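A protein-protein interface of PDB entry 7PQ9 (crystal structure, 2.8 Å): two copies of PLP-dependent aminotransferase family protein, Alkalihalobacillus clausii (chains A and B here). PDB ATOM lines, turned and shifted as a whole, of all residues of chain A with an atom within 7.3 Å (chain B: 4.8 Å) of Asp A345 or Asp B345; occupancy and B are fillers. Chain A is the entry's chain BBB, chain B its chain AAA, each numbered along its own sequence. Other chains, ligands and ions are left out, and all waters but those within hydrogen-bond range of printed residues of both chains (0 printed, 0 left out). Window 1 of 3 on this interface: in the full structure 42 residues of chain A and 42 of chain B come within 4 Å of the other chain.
The backbone NH of Arg B343 is in hydrogen-bond range of the backbone carbonyl oxygen of Ser A314 (3.1 Å).
OD1 of Asp B345 sits close to OD2 of Asp A345 (3.1 Å).
Among the printed residues, merely in contact across the chains: Ser A314 with Ser B342 (3.2 Å), Ser A314 with Ile B344 (3.3 Å), Val A315 with Ser B342 (3.8 Å) and Ser A342 with Val B315 (3.8 Å).
Val A315 touches Ser B342, and with the chains exchanged Ser A342 touches Val B315.
Asp A345 touches its own counterpart, Asp B345.
Positions printed for both chains: 315, 317, 342, 343, 344, 345, 346, 347, 348, 349 and 350.
Of the 6 pairs that touch across the chains among the printed residues, 3 have their exchanged pair printed and touching as well.
Of the printed residues of chain B, Ser A314 touches Ser B342 (3.2 Å), Arg B343 (3.1 Å) and Ile B344 (3.3 Å).
Of the printed residues of chain B, Val A315 touches Ser B342.
Of the printed residues of chain A, Val B315 touches Ser A342 (3.8 Å).
Of chain A, only Asp A345 (3.1 Å) comes within 4 Å of Asp B345.
Thr B350 touches none of the printed residues of chain A.
The nearest residue of chain B that does not touch Asp A345 is Ser B342 (4.3 Å).
The nearest residue of chain A that does not touch Asp B345 is Ser A342 (4.3 Å).
OG of Ser B342 sits close to N of Ile B344, at 3.2 Å.
The side-chain hydroxyl (OG) of Ser A342 lies within hydrogen-bond range of the side-chain carboxylate (OD1) of Asp A345 (3.0 Å).
OD1 of Asp B345 sits at hydrogen-bond distance from OG of Ser B342.
The backbone NH of Ile A344 sits close to the side-chain hydroxyl of Ser A342.
Printed residues of chain B that touch a printed residue of chain A: Val B315, Ser B342, Arg B343, Ile B344 and Asp B345.
Hydrophobic or aromatic side chains of chain B that line the printed part of chain A: Ile B344.
Of the 20 printed residues of chain A, 4 touch a printed residue of chain B.
Among the printed residues, 6 pairs touch across the chains.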
ATOM      1  N   TRP A 124       2.687  27.130  25.603  1.00  0.00           N
ATOM      2  CA  TRP A 124       3.846  26.306  25.916  1.00  0.00           C
ATOM      3  C   TRP A 124       4.027  26.273  27.425  1.00  0.00           C
ATOM      4  O   TRP A 124       4.156  25.207  28.048  1.00  0.00           O
ATOM      5  CB  TRP A 124       5.107  26.753  25.170  1.00  0.00           C
ATOM      6  CG  TRP A 124       6.192  25.704  25.208  1.00  0.00           C
ATOM      7  CD1 TRP A 124       7.225  25.616  26.098  1.00  0.00           C
ATOM      8  CD2 TRP A 124       6.326  24.558  24.347  1.00  0.00           C
ATOM      9  NE1 TRP A 124       8.006  24.529  25.837  1.00  0.00           N
ATOM     10  CE2 TRP A 124       7.473  23.858  24.771  1.00  0.00           C
ATOM     11  CE3 TRP A 124       5.607  24.077  23.245  1.00  0.00           C
ATOM     12  CZ2 TRP A 124       7.905  22.696  24.137  1.00  0.00           C
ATOM     13  CZ3 TRP A 124       6.064  22.953  22.595  1.00  0.00           C
ATOM     14  CH2 TRP A 124       7.176  22.254  23.061  1.00  0.00           C
ATOM     15  N   PHE A 128       3.875  23.260  30.061  1.00  0.00           N
ATOM     16  CA  PHE A 128       4.993  23.068  30.969  1.00  0.00           C
ATOM     17  C   PHE A 128       4.478  22.890  32.397  1.00  0.00           C
ATOM     18  O   PHE A 128       4.846  21.920  33.085  1.00  0.00           O
ATOM     19  CB  PHE A 128       6.051  24.166  30.871  1.00  0.00           C
ATOM     20  CG  PHE A 128       7.277  23.796  31.673  1.00  0.00           C
ATOM     21  CD1 PHE A 128       7.374  24.092  33.020  1.00  0.00           C
ATOM     22  CD2 PHE A 128       8.302  23.069  31.096  1.00  0.00           C
ATOM     23  CE1 PHE A 128       8.472  23.683  33.759  1.00  0.00           C
ATOM     24  CE2 PHE A 128       9.397  22.665  31.833  1.00  0.00           C
ATOM     25  CZ  PHE A 128       9.459  22.937  33.176  1.00  0.00           C
ATOM     26  N   THR A 131       2.872  19.591  33.012  1.00  0.00           N
ATOM     27  CA  THR A 131       3.757  18.437  33.024  1.00  0.00           C
ATOM     28  C   THR A 131       4.699  18.426  34.233  1.00  0.00           C
ATOM     29  O   THR A 131       4.901  17.369  34.849  1.00  0.00           O
ATOM     30  CB  THR A 131       4.682  18.451  31.812  1.00  0.00           C
ATOM     31  OG1 THR A 131       3.856  18.813  30.714  1.00  0.00           O
ATOM     32  CG2 THR A 131       5.372  17.123  31.584  1.00  0.00           C
ATOM     33  N   PHE A 151       5.093   9.930  22.942  1.00  0.00           N
ATOM     34  CA  PHE A 151       5.585  10.984  22.074  1.00  0.00           C
ATOM     35  C   PHE A 151       5.819  10.369  20.703  1.00  0.00           C
ATOM     36  O   PHE A 151       5.534  10.980  19.678  1.00  0.00           O
ATOM     37  CB  PHE A 151       6.778  11.713  22.713  1.00  0.00           C
ATOM     38  CG  PHE A 151       7.437  12.755  21.837  1.00  0.00           C
ATOM     39  CD1 PHE A 151       6.694  13.672  21.131  1.00  0.00           C
ATOM     40  CD2 PHE A 151       8.814  12.812  21.693  1.00  0.00           C
ATOM     41  CE1 PHE A 151       7.325  14.613  20.313  1.00  0.00           C
ATOM     42  CE2 PHE A 151       9.423  13.753  20.882  1.00  0.00           C
ATOM     43  CZ  PHE A 151       8.686  14.661  20.194  1.00  0.00           C
ATOM     44  N   LEU A 311       7.632  24.527  15.414  1.00  0.00           N
ATOM     45  CA  LEU A 311       8.109  24.626  16.803  1.00  0.00           C
ATOM     46  C   LEU A 311       9.366  25.503  17.048  1.00  0.00           C
ATOM     47  O   LEU A 311       9.350  26.702  16.775  1.00  0.00           O
ATOM     48  CB  LEU A 311       8.284  23.235  17.397  1.00  0.00           C
ATOM     49  CG  LEU A 311       7.855  23.183  18.863  1.00  0.00           C
ATOM     50  CD1 LEU A 311       6.348  23.435  19.048  1.00  0.00           C
ATOM     51  CD2 LEU A 311       8.290  21.876  19.509  1.00  0.00           C
ATOM     52  N   ILE A 312      10.421  24.935  17.658  1.00  0.00           N
ATOM     53  CA  ILE A 312      11.521  25.681  18.285  1.00  0.00           C
ATOM     54  C   ILE A 312      12.893  25.055  18.013  1.00  0.00           C
ATOM     55  O   ILE A 312      13.245  24.059  18.672  1.00  0.00           O
ATOM     56  CB  ILE A 312      11.376  25.644  19.820  1.00  0.00           C
ATOM     57  CG1 ILE A 312      10.043  26.175  20.339  1.00  0.00           C
ATOM     58  CG2 ILE A 312      12.545  26.410  20.441  1.00  0.00           C
ATOM     59  CD1 ILE A 312       9.796  25.793  21.794  1.00  0.00           C
ATOM     60  N   SER A 314      15.847  25.432  19.148  1.00  0.00           N
ATOM     61  CA  SER A 314      16.845  25.345  20.205  1.00  0.00           C
ATOM     62  C   SER A 314      16.478  24.279  21.238  1.00  0.00           C
ATOM     63  O   SER A 314      17.245  24.038  22.178  1.00  0.00           O
ATOM     64  CB  SER A 314      17.065  26.690  20.830  1.00  0.00           C
ATOM     65  OG  SER A 314      16.022  26.971  21.744  1.00  0.00           O
ATOM     66  N   VAL A 315      15.322  23.623  21.052  1.00  0.00           N
ATOM     67  CA  VAL A 315      14.905  22.597  21.994  1.00  0.00           C
ATOM     68  C   VAL A 315      15.586  21.267  21.649  1.00  0.00           C
ATOM     69  O   VAL A 315      15.567  20.311  22.462  1.00  0.00           O
ATOM     70  CB  VAL A 315      13.384  22.417  22.063  1.00  0.00           C
ATOM     71  CG1 VAL A 315      13.077  21.434  23.173  1.00  0.00           C
ATOM     72  CG2 VAL A 315      12.723  23.717  22.413  1.00  0.00           C
ATOM     73  N   ILE A 317      14.877  18.784  19.307  1.00  0.00           N
ATOM     74  CA  ILE A 317      14.079  17.568  19.246  1.00  0.00           C
ATOM     75  C   ILE A 317      13.943  17.089  17.808  1.00  0.00           C
ATOM     76  O   ILE A 317      13.377  17.776  16.984  1.00  0.00           O
ATOM     77  CB  ILE A 317      12.739  17.720  19.929  1.00  0.00           C
ATOM     78  CG1 ILE A 317      12.901  18.052  21.413  1.00  0.00           C
ATOM     79  CG2 ILE A 317      11.971  16.421  19.764  1.00  0.00           C
ATOM     80  CD1 ILE A 317      11.587  18.569  22.043  1.00  0.00           C
ATOM     81  N   VAL A 341      16.951  13.411  24.794  1.00  0.00           N
ATOM     82  CA  VAL A 341      15.967  14.493  24.806  1.00  0.00           C
ATOM     83  C   VAL A 341      15.218  14.466  26.120  1.00  0.00           C
ATOM     84  O   VAL A 341      14.906  13.389  26.653  1.00  0.00           O
ATOM     85  CB  VAL A 341      14.980  14.408  23.630  1.00  0.00           C
ATOM     86  CG1 VAL A 341      13.867  15.452  23.698  1.00  0.00           C
ATOM     87  CG2 VAL A 341      15.692  14.435  22.264  1.00  0.00           C
ATOM     88  N   SER A 342      14.992  15.668  26.667  1.00  0.00           N
ATOM     89  CA  SER A 342      14.419  15.726  28.004  1.00  0.00           C
ATOM     90  C   SER A 342      13.038  15.062  28.004  1.00  0.00           C
ATOM     91  O   SER A 342      12.204  15.459  27.204  1.00  0.00           O
ATOM     92  CB  SER A 342      14.301  17.148  28.402  1.00  0.00           C
ATOM     93  OG  SER A 342      13.535  17.255  29.597  1.00  0.00           O
ATOM     94  N   ARG A 343      12.774  14.116  28.916  1.00  0.00           N
ATOM     95  CA  ARG A 343      11.426  13.585  29.114  1.00  0.00           C
ATOM     96  C   ARG A 343      10.426  14.721  29.294  1.00  0.00           C
ATOM     97  O   ARG A 343       9.345  14.660  28.722  1.00  0.00           O
ATOM     98  CB  ARG A 343      11.282  12.824  30.435  1.00  0.00           C
ATOM     99  CG  ARG A 343      11.554  11.347  30.334  1.00  0.00           C
ATOM    100  CD  ARG A 343      10.300  10.612  30.725  1.00  0.00           C
ATOM    101  NE  ARG A 343      10.478   9.845  31.941  1.00  0.00           N
ATOM    102  CZ  ARG A 343       9.641   8.895  32.338  1.00  0.00           C
ATOM    103  NH1 ARG A 343       9.848   8.244  33.462  1.00  0.00           N
ATOM    104  NH2 ARG A 343       8.578   8.616  31.608  1.00  0.00           N
ATOM    105  N   ILE A 344      10.756  15.710  30.139  1.00  0.00           N
ATOM    106  CA  ILE A 344       9.808  16.769  30.398  1.00  0.00           C
ATOM    107  C   ILE A 344       9.413  17.396  29.063  1.00  0.00           C
ATOM    108  O   ILE A 344       8.218  17.650  28.825  1.00  0.00           O
ATOM    109  CB  ILE A 344      10.353  17.800  31.411  1.00  0.00           C
ATOM    110  CG1 ILE A 344      10.664  17.219  32.785  1.00  0.00           C
ATOM    111  CG2 ILE A 344       9.472  19.033  31.510  1.00  0.00           C
ATOM    112  CD1 ILE A 344       9.462  16.671  33.544  1.00  0.00           C
ATOM    113  N   ASP A 345      10.406  17.610  28.183  1.00  0.00           N
ATOM    114  CA  ASP A 345      10.143  18.387  26.980  1.00  0.00           C
ATOM    115  C   ASP A 345       9.313  17.506  26.047  1.00  0.00           C
ATOM    116  O   ASP A 345       8.379  17.979  25.402  1.00  0.00           O
ATOM    117  CB  ASP A 345      11.399  19.042  26.374  1.00  0.00           C
ATOM    118  CG  ASP A 345      12.108  20.078  27.257  1.00  0.00           C
ATOM    119  OD1 ASP A 345      12.466  19.762  28.420  1.00  0.00           O
ATOM    120  OD2 ASP A 345      12.343  21.191  26.783  1.00  0.00           O
ATOM    121  N   GLN A 346       9.603  16.197  26.069  1.00  0.00           N
ATOM    122  CA  GLN A 346       8.870  15.226  25.276  1.00  0.00           C
ATOM    123  C   GLN A 346       7.393  15.265  25.674  1.00  0.00           C
ATOM    124  O   GLN A 346       6.531  15.439  24.818  1.00  0.00           O
ATOM    125  CB  GLN A 346       9.443  13.820  25.455  1.00  0.00           C
ATOM    126  CG  GLN A 346      10.718  13.584  24.676  1.00  0.00           C
ATOM    127  CD  GLN A 346      11.167  12.155  24.783  1.00  0.00           C
ATOM    128  OE1 GLN A 346      10.618  11.261  24.170  1.00  0.00           O
ATOM    129  NE2 GLN A 346      12.210  11.926  25.523  1.00  0.00           N
ATOM    130  N   GLN A 347       7.122  15.101  26.972  1.00  0.00           N
ATOM    131  CA  GLN A 347       5.776  15.145  27.519  1.00  0.00           C
ATOM    132  C   GLN A 347       5.063  16.446  27.160  1.00  0.00           C
ATOM    133  O   GLN A 347       3.899  16.420  26.741  1.00  0.00           O
ATOM    134  CB  GLN A 347       5.785  14.912  29.019  1.00  0.00           C
ATOM    135  CG  GLN A 347       6.042  13.451  29.415  1.00  0.00           C
ATOM    136  CD  GLN A 347       5.089  12.477  28.755  1.00  0.00           C
ATOM    137  OE1 GLN A 347       3.961  12.811  28.412  1.00  0.00           O
ATOM    138  NE2 GLN A 347       5.546  11.252  28.566  1.00  0.00           N
ATOM    139  N   VAL A 348       5.761  17.576  27.320  1.00  0.00           N
ATOM    140  CA  VAL A 348       5.173  18.860  26.989  1.00  0.00           C
ATOM    141  C   VAL A 348       4.756  18.843  25.530  1.00  0.00           C
ATOM    142  O   VAL A 348       3.610  19.143  25.231  1.00  0.00           O
ATOM    143  CB  VAL A 348       6.132  20.024  27.320  1.00  0.00           C
ATOM    144  CG1 VAL A 348       5.825  21.323  26.556  1.00  0.00           C
ATOM    145  CG2 VAL A 348       6.181  20.272  28.812  1.00  0.00           C
ATOM    146  N   LEU A 349       5.678  18.505  24.628  1.00  0.00           N
ATOM    147  CA  LEU A 349       5.381  18.553  23.196  1.00  0.00           C
ATOM    148  C   LEU A 349       4.286  17.533  22.863  1.00  0.00           C
ATOM    149  O   LEU A 349       3.463  17.796  22.011  1.00  0.00           O
ATOM    150  CB  LEU A 349       6.656  18.262  22.404  1.00  0.00           C
ATOM    151  CG  LEU A 349       6.513  18.335  20.902  1.00  0.00           C
ATOM    152  CD1 LEU A 349       5.740  19.567  20.478  1.00  0.00           C
ATOM    153  CD2 LEU A 349       7.876  18.245  20.158  1.00  0.00           C
ATOM    154  N   THR A 350       4.293  16.386  23.556  1.00  0.00           N
ATOM    155  CA  THR A 350       3.270  15.364  23.395  1.00  0.00           C
ATOM    156  C   THR A 350       1.900  15.994  23.614  1.00  0.00           C
ATOM    157  O   THR A 350       1.065  15.944  22.723  1.00  0.00           O
ATOM    158  CB  THR A 350       3.481  14.167  24.331  1.00  0.00           C
ATOM    159  OG1 THR A 350       4.697  13.466  24.046  1.00  0.00           O
ATOM    160  CG2 THR A 350       2.343  13.189  24.300  1.00  0.00           C
ATOM    161  N   ALA A 351       1.703  16.630  24.775  1.00  0.00           N
ATOM    162  CA  ALA A 351       0.446  17.316  25.088  1.00  0.00           C
ATOM    163  C   ALA A 351       0.125  18.374  24.026  1.00  0.00           C
ATOM    164  O   ALA A 351      -0.975  18.417  23.491  1.00  0.00           O
ATOM    165  CB  ALA A 351       0.510  17.950  26.445  1.00  0.00           C
ATOM    166  N   VAL B 315      16.522  15.212  32.375  1.00  0.00           N
ATOM    167  CA  VAL B 315      16.695  16.434  31.612  1.00  0.00           C
ATOM    168  C   VAL B 315      17.883  16.300  30.661  1.00  0.00           C
ATOM    169  O   VAL B 315      18.055  17.119  29.728  1.00  0.00           O
ATOM    170  CB  VAL B 315      16.841  17.685  32.483  1.00  0.00           C
ATOM    171  CG1 VAL B 315      16.839  18.894  31.551  1.00  0.00           C
ATOM    172  CG2 VAL B 315      15.654  17.814  33.414  1.00  0.00           C
ATOM    173  N   ILE B 317      21.321  16.680  31.116  1.00  0.00           N
ATOM    174  CA  ILE B 317      22.290  17.766  31.045  1.00  0.00           C
ATOM    175  C   ILE B 317      23.600  17.345  31.693  1.00  0.00           C
ATOM    176  O   ILE B 317      23.649  17.061  32.895  1.00  0.00           O
ATOM    177  CB  ILE B 317      21.755  19.058  31.650  1.00  0.00           C
ATOM    178  CG1 ILE B 317      20.523  19.554  30.885  1.00  0.00           C
ATOM    179  CG2 ILE B 317      22.859  20.093  31.619  1.00  0.00           C
ATOM    180  CD1 ILE B 317      19.766  20.657  31.614  1.00  0.00           C
ATOM    181  N   SER B 342      18.756  21.637  25.341  1.00  0.00           N
ATOM    182  CA  SER B 342      17.863  22.742  25.044  1.00  0.00           C
ATOM    183  C   SER B 342      18.425  24.047  25.617  1.00  0.00           C
ATOM    184  O   SER B 342      18.690  24.087  26.814  1.00  0.00           O
ATOM    185  CB  SER B 342      16.543  22.455  25.669  1.00  0.00           C
ATOM    186  OG  SER B 342      15.702  23.608  25.582  1.00  0.00           O
ATOM    187  N   ARG B 343      18.554  25.105  24.804  1.00  0.00           N
ATOM    188  CA  ARG B 343      18.887  26.426  25.326  1.00  0.00           C
ATOM    189  C   ARG B 343      17.949  26.818  26.474  1.00  0.00           C
ATOM    190  O   ARG B 343      18.413  27.347  27.478  1.00  0.00           O
ATOM    191  CB  ARG B 343      18.660  27.573  24.363  1.00  0.00           C
ATOM    192  CG  ARG B 343      19.813  27.855  23.434  1.00  0.00           C
ATOM    193  CD  ARG B 343      20.115  29.324  23.644  1.00  0.00           C
ATOM    194  NE  ARG B 343      19.867  30.143  22.463  1.00  0.00           N
ATOM    195  CZ  ARG B 343      20.323  31.362  22.311  1.00  0.00           C
ATOM    196  NH1 ARG B 343      20.048  32.032  21.212  1.00  0.00           N
ATOM    197  NH2 ARG B 343      21.070  31.909  23.251  1.00  0.00           N
ATOM    198  N   ILE B 344      16.644  26.610  26.316  1.00  0.00           N
ATOM    199  CA  ILE B 344      15.723  27.022  27.352  1.00  0.00           C
ATOM    200  C   ILE B 344      16.133  26.347  28.657  1.00  0.00           C
ATOM    201  O   ILE B 344      16.136  27.003  29.707  1.00  0.00           O
ATOM    202  CB  ILE B 344      14.249  26.787  26.944  1.00  0.00           C
ATOM    203  CG1 ILE B 344      13.838  27.801  25.878  1.00  0.00           C
ATOM    204  CG2 ILE B 344      13.267  26.863  28.109  1.00  0.00           C
ATOM    205  CD1 ILE B 344      14.247  27.325  24.528  1.00  0.00           C
ATOM    206  N   ASP B 345      16.506  25.063  28.582  1.00  0.00           N
ATOM    207  CA  ASP B 345      16.729  24.303  29.807  1.00  0.00           C
ATOM    208  C   ASP B 345      18.039  24.793  30.415  1.00  0.00           C
ATOM    209  O   ASP B 345      18.147  24.955  31.635  1.00  0.00           O
ATOM    210  CB  ASP B 345      16.576  22.784  29.650  1.00  0.00           C
ATOM    211  CG  ASP B 345      15.178  22.291  29.261  1.00  0.00           C
ATOM    212  OD1 ASP B 345      14.642  22.747  28.206  1.00  0.00           O
ATOM    213  OD2 ASP B 345      14.622  21.441  30.021  1.00  0.00           O
ATOM    214  N   GLN B 346      18.990  25.135  29.534  1.00  0.00           N
ATOM    215  CA  GLN B 346      20.274  25.674  29.956  1.00  0.00           C
ATOM    216  C   GLN B 346      20.042  26.955  30.742  1.00  0.00           C
ATOM    217  O   GLN B 346      20.523  27.074  31.872  1.00  0.00           O
ATOM    218  CB  GLN B 346      21.188  25.911  28.750  1.00  0.00           C
ATOM    219  CG  GLN B 346      21.827  24.640  28.215  1.00  0.00           C
ATOM    220  CD  GLN B 346      22.819  24.946  27.130  1.00  0.00           C
ATOM    221  OE1 GLN B 346      23.909  25.448  27.366  1.00  0.00           O
ATOM    222  NE2 GLN B 346      22.464  24.629  25.921  1.00  0.00           N
ATOM    223  N   GLN B 347      19.314  27.905  30.127  1.00  0.00           N
ATOM    224  CA  GLN B 347      18.974  29.181  30.749  1.00  0.00           C
ATOM    225  C   GLN B 347      18.274  28.976  32.092  1.00  0.00           C
ATOM    226  O   GLN B 347      18.615  29.633  33.073  1.00  0.00           O
ATOM    227  CB  GLN B 347      18.151  30.039  29.808  1.00  0.00           C
ATOM    228  CG  GLN B 347      18.956  30.662  28.660  1.00  0.00           C
ATOM    229  CD  GLN B 347      20.132  31.469  29.138  1.00  0.00           C
ATOM    230  OE1 GLN B 347      20.106  32.017  30.246  1.00  0.00           O
ATOM    231  NE2 GLN B 347      21.160  31.559  28.294  1.00  0.00           N
ATOM    232  N   VAL B 348      17.303  28.074  32.129  1.00  0.00           N
ATOM    233  CA  VAL B 348      16.579  27.799  33.352  1.00  0.00           C
ATOM    234  C   VAL B 348      17.567  27.361  34.419  1.00  0.00           C
ATOM    235  O   VAL B 348      17.586  27.934  35.503  1.00  0.00           O
ATOM    236  CB  VAL B 348      15.445  26.775  33.122  1.00  0.00           C
ATOM    237  CG1 VAL B 348      14.961  26.124  34.414  1.00  0.00           C
ATOM    238  CG2 VAL B 348      14.269  27.423  32.399  1.00  0.00           C
ATOM    239  N   LEU B 349      18.381  26.345  34.117  1.00  0.00           N
ATOM    240  CA  LEU B 349      19.305  25.819  35.119  1.00  0.00           C
ATOM    241  C   LEU B 349      20.332  26.885  35.502  1.00  0.00           C
ATOM    242  O   LEU B 349      20.739  26.946  36.659  1.00  0.00           O
ATOM    243  CB  LEU B 349      20.002  24.577  34.558  1.00  0.00           C
ATOM    244  CG  LEU B 349      20.962  23.885  35.510  1.00  0.00           C
ATOM    245  CD1 LEU B 349      20.325  23.712  36.879  1.00  0.00           C
ATOM    246  CD2 LEU B 349      21.443  22.545  34.942  1.00  0.00           C
ATOM    247  N   THR B 350      20.735  27.714  34.515  1.00  0.00           N
ATOM    248  CA  THR B 350      21.657  28.811  34.754  1.00  0.00           C
ATOM    249  C   THR B 350      21.102  29.682  35.881  1.00  0.00           C
ATOM    250  O   THR B 350      21.763  29.875  36.901  1.00  0.00           O
ATOM    251  CB  THR B 350      21.918  29.643  33.500  1.00  0.00           C
ATOM    252  OG1 THR B 350      22.574  28.925  32.455  1.00  0.00           O
ATOM    253  CG2 THR B 350      22.744  30.857  33.783  1.00  0.00           C
